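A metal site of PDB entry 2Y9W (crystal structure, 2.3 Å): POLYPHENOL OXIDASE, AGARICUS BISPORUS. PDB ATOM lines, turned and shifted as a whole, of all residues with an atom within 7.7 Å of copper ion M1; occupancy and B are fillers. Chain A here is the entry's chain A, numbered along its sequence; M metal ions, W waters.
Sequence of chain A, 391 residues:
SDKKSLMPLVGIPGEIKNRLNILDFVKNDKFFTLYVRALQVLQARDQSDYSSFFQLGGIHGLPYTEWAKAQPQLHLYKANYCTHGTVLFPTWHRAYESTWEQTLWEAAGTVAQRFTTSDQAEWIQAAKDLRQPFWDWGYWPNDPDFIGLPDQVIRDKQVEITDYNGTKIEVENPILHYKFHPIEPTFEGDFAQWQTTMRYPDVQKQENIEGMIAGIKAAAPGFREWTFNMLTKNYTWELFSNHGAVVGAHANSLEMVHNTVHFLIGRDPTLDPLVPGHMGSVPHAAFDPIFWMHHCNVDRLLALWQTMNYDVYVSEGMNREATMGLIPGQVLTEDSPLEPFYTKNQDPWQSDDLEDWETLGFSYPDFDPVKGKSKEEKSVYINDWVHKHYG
The backbone carbonyl oxygen of Glu 255 is in hydrogen-bond range of a ring nitrogen (ND1) of His 258 (3.1 Å).
ND1 of His 262 sits at hydrogen-bond distance from O of Met 279.
A ring nitrogen (NE2) of His 294 sits at hydrogen-bond distance from the backbone carbonyl oxygen (O) of His 258 (3.2 Å).
ND1 of His 258 lies within hydrogen-bond range of OD1 of Asn 259 (3.4 Å).
Copper ion M1 is bound by a ring nitrogen (NE2) of His 295 (2.0 Å), a ring nitrogen (NE2) of His 262 (2.1 Å) and a ring nitrogen (NE2) of His 258 (2.1 Å).
Slightly farther from copper ion M1 lies water W1 (2.6 Å).
Phe 291 touches copper ion M1.
Four residues have an atom within 4 Å of copper ion M1: His 258, His 262, Phe 291 and His 295.
The nearest printed residue that does not touch copper ion M1 is His 294 (4.03 Å).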
ATOM      1  N   HIS A  60     -18.097  -2.564   3.985  1.00  0.00           N
ATOM      2  CA  HIS A  60     -19.279  -1.739   3.772  1.00  0.00           C
ATOM      3  C   HIS A  60     -19.393  -1.276   2.322  1.00  0.00           C
ATOM      4  O   HIS A  60     -20.401  -1.560   1.658  1.00  0.00           O
ATOM      5  CB  HIS A  60     -19.226  -0.559   4.741  1.00  0.00           C
ATOM      6  CG  HIS A  60     -20.459   0.282   4.768  1.00  0.00           C
ATOM      7  ND1 HIS A  60     -20.526   1.514   4.153  1.00  0.00           N
ATOM      8  CD2 HIS A  60     -21.668   0.096   5.360  1.00  0.00           C
ATOM      9  CE1 HIS A  60     -21.728   2.037   4.342  1.00  0.00           C
ATOM     10  NE2 HIS A  60     -22.437   1.196   5.074  1.00  0.00           N
ATOM     11  N   HIS A  84     -28.749  -1.258   1.244  1.00  0.00           N
ATOM     12  CA  HIS A  84     -29.410   0.002   1.580  1.00  0.00           C
ATOM     13  C   HIS A  84     -30.642   0.099   0.684  1.00  0.00           C
ATOM     14  O   HIS A  84     -30.654  -0.470  -0.407  1.00  0.00           O
ATOM     15  CB  HIS A  84     -28.447   1.205   1.392  1.00  0.00           C
ATOM     16  CG  HIS A  84     -27.132   1.049   2.102  1.00  0.00           C
ATOM     17  ND1 HIS A  84     -26.025   0.484   1.519  1.00  0.00           N
ATOM     18  CD2 HIS A  84     -26.764   1.378   3.367  1.00  0.00           C
ATOM     19  CE1 HIS A  84     -25.018   0.468   2.378  1.00  0.00           C
ATOM     20  NE2 HIS A  84     -25.441   1.014   3.516  1.00  0.00           N
ATOM     21  N   PHE A  89     -31.931  -3.753   5.367  1.00  0.00           N
ATOM     22  CA  PHE A  89     -31.022  -2.725   5.894  1.00  0.00           C
ATOM     23  C   PHE A  89     -30.698  -2.883   7.390  1.00  0.00           C
ATOM     24  O   PHE A  89     -29.524  -2.878   7.741  1.00  0.00           O
ATOM     25  CB  PHE A  89     -31.510  -1.295   5.572  1.00  0.00           C
ATOM     26  CG  PHE A  89     -30.880  -0.243   6.446  1.00  0.00           C
ATOM     27  CD1 PHE A  89     -29.627   0.264   6.132  1.00  0.00           C
ATOM     28  CD2 PHE A  89     -31.527   0.210   7.601  1.00  0.00           C
ATOM     29  CE1 PHE A  89     -29.026   1.213   6.946  1.00  0.00           C
ATOM     30  CE2 PHE A  89     -30.930   1.152   8.430  1.00  0.00           C
ATOM     31  CZ  PHE A  89     -29.672   1.654   8.096  1.00  0.00           C
ATOM     32  N   HIS A  93     -26.908  -4.667   8.900  1.00  0.00           N
ATOM     33  CA  HIS A  93     -26.079  -3.782   9.713  1.00  0.00           C
ATOM     34  C   HIS A  93     -25.872  -4.247  11.149  1.00  0.00           C
ATOM     35  O   HIS A  93     -24.839  -3.950  11.726  1.00  0.00           O
ATOM     36  CB  HIS A  93     -26.586  -2.348   9.653  1.00  0.00           C
ATOM     37  CG  HIS A  93     -26.204  -1.642   8.403  1.00  0.00           C
ATOM     38  ND1 HIS A  93     -27.024  -1.585   7.297  1.00  0.00           N
ATOM     39  CD2 HIS A  93     -25.073  -0.979   8.066  1.00  0.00           C
ATOM     40  CE1 HIS A  93     -26.415  -0.899   6.333  1.00  0.00           C
ATOM     41  NE2 HIS A  93     -25.228  -0.522   6.787  1.00  0.00           N
ATOM     42  N   GLU A 255     -33.943   4.062   8.397  1.00  0.00           N
ATOM     43  CA  GLU A 255     -32.880   4.300   7.430  1.00  0.00           C
ATOM     44  C   GLU A 255     -32.762   5.787   7.100  1.00  0.00           C
ATOM     45  O   GLU A 255     -31.656   6.323   7.033  1.00  0.00           O
ATOM     46  CB  GLU A 255     -33.062   3.449   6.171  1.00  0.00           C
ATOM     47  CG  GLU A 255     -31.967   3.666   5.156  1.00  0.00           C
ATOM     48  CD  GLU A 255     -31.952   2.649   4.042  1.00  0.00           C
ATOM     49  OE1 GLU A 255     -33.036   2.224   3.592  1.00  0.00           O
ATOM     50  OE2 GLU A 255     -30.847   2.279   3.602  1.00  0.00           O
ATOM     51  N   HIS A 258     -31.338   7.804   9.988  1.00  0.00           N
ATOM     52  CA  HIS A 258     -29.926   7.405   9.899  1.00  0.00           C
ATOM     53  C   HIS A 258     -29.143   8.042   8.726  1.00  0.00           C
ATOM     54  O   HIS A 258     -27.956   8.306   8.858  1.00  0.00           O
ATOM     55  CB  HIS A 258     -29.829   5.857   9.887  1.00  0.00           C
ATOM     56  CG  HIS A 258     -28.740   5.293   9.019  1.00  0.00           C
ATOM     57  ND1 HIS A 258     -28.872   5.141   7.656  1.00  0.00           N
ATOM     58  CD2 HIS A 258     -27.504   4.809   9.331  1.00  0.00           C
ATOM     59  CE1 HIS A 258     -27.768   4.609   7.156  1.00  0.00           C
ATOM     60  NE2 HIS A 258     -26.927   4.386   8.151  1.00  0.00           N
ATOM     61  N   ASN A 259     -29.804   8.286   7.593  1.00  0.00           N
ATOM     62  CA  ASN A 259     -29.161   8.960   6.459  1.00  0.00           C
ATOM     63  C   ASN A 259     -28.737  10.390   6.838  1.00  0.00           C
ATOM     64  O   ASN A 259     -27.591  10.785   6.665  1.00  0.00           O
ATOM     65  CB  ASN A 259     -30.086   8.997   5.220  1.00  0.00           C
ATOM     66  CG  ASN A 259     -30.208   7.645   4.519  1.00  0.00           C
ATOM     67  OD1 ASN A 259     -29.384   6.752   4.698  1.00  0.00           O
ATOM     68  ND2 ASN A 259     -31.249   7.493   3.706  1.00  0.00           N
ATOM     69  N   VAL A 261     -28.205  11.621   9.749  1.00  0.00           N
ATOM     70  CA  VAL A 261     -27.115  11.612  10.728  1.00  0.00           C
ATOM     71  C   VAL A 261     -25.737  11.532  10.057  1.00  0.00           C
ATOM     72  O   VAL A 261     -24.814  12.259  10.439  1.00  0.00           O
ATOM     73  CB  VAL A 261     -27.282  10.530  11.812  1.00  0.00           C
ATOM     74  CG1 VAL A 261     -26.038  10.435  12.672  1.00  0.00           C
ATOM     75  CG2 VAL A 261     -28.486  10.817  12.694  1.00  0.00           C
ATOM     76  N   HIS A 262     -25.607  10.671   9.040  1.00  0.00           N
ATOM     77  CA  HIS A 262     -24.395  10.609   8.218  1.00  0.00           C
ATOM     78  C   HIS A 262     -24.028  11.987   7.664  1.00  0.00           C
ATOM     79  O   HIS A 262     -22.862  12.358   7.657  1.00  0.00           O
ATOM     80  CB  HIS A 262     -24.578   9.648   7.063  1.00  0.00           C
ATOM     81  CG  HIS A 262     -24.240   8.233   7.384  1.00  0.00           C
ATOM     82  ND1 HIS A 262     -22.947   7.749   7.318  1.00  0.00           N
ATOM     83  CD2 HIS A 262     -25.014   7.184   7.754  1.00  0.00           C
ATOM     84  CE1 HIS A 262     -22.937   6.467   7.640  1.00  0.00           C
ATOM     85  NE2 HIS A 262     -24.179   6.095   7.918  1.00  0.00           N
ATOM     86  N   MET A 279     -17.932  10.103   6.007  1.00  0.00           N
ATOM     87  CA  MET A 279     -19.248   9.787   6.585  1.00  0.00           C
ATOM     88  C   MET A 279     -20.449  10.242   5.743  1.00  0.00           C
ATOM     89  O   MET A 279     -21.535   9.705   5.889  1.00  0.00           O
ATOM     90  CB  MET A 279     -19.348  10.301   8.016  1.00  0.00           C
ATOM     91  CG  MET A 279     -18.684   9.386   9.037  1.00  0.00           C
ATOM     92  SD  MET A 279     -19.714   7.965   9.476  1.00  0.00           S
ATOM     93  CE  MET A 279     -21.027   8.774  10.396  1.00  0.00           C
ATOM     94  N   VAL A 282     -21.532   6.843   1.139  1.00  0.00           N
ATOM     95  CA  VAL A 282     -21.777   5.411   1.421  1.00  0.00           C
ATOM     96  C   VAL A 282     -20.564   4.485   1.140  1.00  0.00           C
ATOM     97  O   VAL A 282     -20.246   3.612   1.958  1.00  0.00           O
ATOM     98  CB  VAL A 282     -23.086   4.865   0.722  1.00  0.00           C
ATOM     99  CG1 VAL A 282     -23.318   3.401   1.064  1.00  0.00           C
ATOM    100  CG2 VAL A 282     -24.302   5.694   1.113  1.00  0.00           C
ATOM    101  N   ALA A 285     -17.889   5.717   4.179  1.00  0.00           N
ATOM    102  CA  ALA A 285     -18.306   6.050   5.546  1.00  0.00           C
ATOM    103  C   ALA A 285     -17.677   5.183   6.640  1.00  0.00           C
ATOM    104  O   ALA A 285     -17.293   5.694   7.700  1.00  0.00           O
ATOM    105  CB  ALA A 285     -19.830   6.028   5.659  1.00  0.00           C
ATOM    106  N   ALA A 286     -17.538   3.897   6.357  1.00  0.00           N
ATOM    107  CA  ALA A 286     -17.179   2.915   7.379  1.00  0.00           C
ATOM    108  C   ALA A 286     -15.734   2.995   7.857  1.00  0.00           C
ATOM    109  O   ALA A 286     -15.366   2.291   8.806  1.00  0.00           O
ATOM    110  CB  ALA A 286     -17.508   1.528   6.888  1.00  0.00           C
ATOM    111  N   PHE A 291     -18.466   5.909  12.666  1.00  0.00           N
ATOM    112  CA  PHE A 291     -19.416   5.027  11.973  1.00  0.00           C
ATOM    113  C   PHE A 291     -19.993   3.994  12.953  1.00  0.00           C
ATOM    114  O   PHE A 291     -21.206   3.756  12.946  1.00  0.00           O
ATOM    115  CB  PHE A 291     -18.733   4.298  10.798  1.00  0.00           C
ATOM    116  CG  PHE A 291     -19.658   3.426   9.991  1.00  0.00           C
ATOM    117  CD1 PHE A 291     -20.397   3.959   8.919  1.00  0.00           C
ATOM    118  CD2 PHE A 291     -19.805   2.072  10.292  1.00  0.00           C
ATOM    119  CE1 PHE A 291     -21.274   3.159   8.160  1.00  0.00           C
ATOM    120  CE2 PHE A 291     -20.662   1.252   9.550  1.00  0.00           C
ATOM    121  CZ  PHE A 291     -21.403   1.797   8.470  1.00  0.00           C
ATOM    122  N   HIS A 294     -22.394   5.423  15.559  1.00  0.00           N
ATOM    123  CA  HIS A 294     -23.628   5.753  14.859  1.00  0.00           C
ATOM    124  C   HIS A 294     -24.446   4.484  14.655  1.00  0.00           C
ATOM    125  O   HIS A 294     -25.633   4.436  14.984  1.00  0.00           O
ATOM    126  CB  HIS A 294     -23.296   6.394  13.509  1.00  0.00           C
ATOM    127  CG  HIS A 294     -24.484   6.673  12.643  1.00  0.00           C
ATOM    128  ND1 HIS A 294     -25.721   7.003  13.159  1.00  0.00           N
ATOM    129  CD2 HIS A 294     -24.615   6.724  11.301  1.00  0.00           C
ATOM    130  CE1 HIS A 294     -26.560   7.215  12.171  1.00  0.00           C
ATOM    131  NE2 HIS A 294     -25.908   7.072  11.026  1.00  0.00           N
ATOM    132  N   HIS A 295     -23.776   3.446  14.160  1.00  0.00           N
ATOM    133  CA  HIS A 295     -24.451   2.193  13.905  1.00  0.00           C
ATOM    134  C   HIS A 295     -24.829   1.391  15.108  1.00  0.00           C
ATOM    135  O   HIS A 295     -25.835   0.675  15.088  1.00  0.00           O
ATOM    136  CB  HIS A 295     -23.720   1.379  12.866  1.00  0.00           C
ATOM    137  CG  HIS A 295     -24.174   1.724  11.501  1.00  0.00           C
ATOM    138  ND1 HIS A 295     -25.322   1.185  10.950  1.00  0.00           N
ATOM    139  CD2 HIS A 295     -23.742   2.659  10.631  1.00  0.00           C
ATOM    140  CE1 HIS A 295     -25.524   1.719   9.763  1.00  0.00           C
ATOM    141  NE2 HIS A 295     -24.573   2.612   9.544  1.00  0.00           N
ATOM    142  N   VAL A 298     -28.222   2.951  15.719  1.00  0.00           N
ATOM    143  CA  VAL A 298     -29.158   2.356  14.761  1.00  0.00           C
ATOM    144  C   VAL A 298     -29.600   0.921  15.186  1.00  0.00           C
ATOM    145  O   VAL A 298     -30.770   0.558  15.036  1.00  0.00           O
ATOM    146  CB  VAL A 298     -28.563   2.296  13.322  1.00  0.00           C
ATOM    147  CG1 VAL A 298     -29.487   1.562  12.365  1.00  0.00           C
ATOM    148  CG2 VAL A 298     -28.263   3.689  12.817  1.00  0.00           C
HETATM  149 CU    CU M   1     -24.855   4.146   8.214  1.00  0.00          CU
HETATM  150 CU    CU M   2     -24.443   0.727   5.336  1.00  0.00          CU
HETATM  151  O   HOH W   1     -25.303   3.583   5.680  1.00  0.00           O
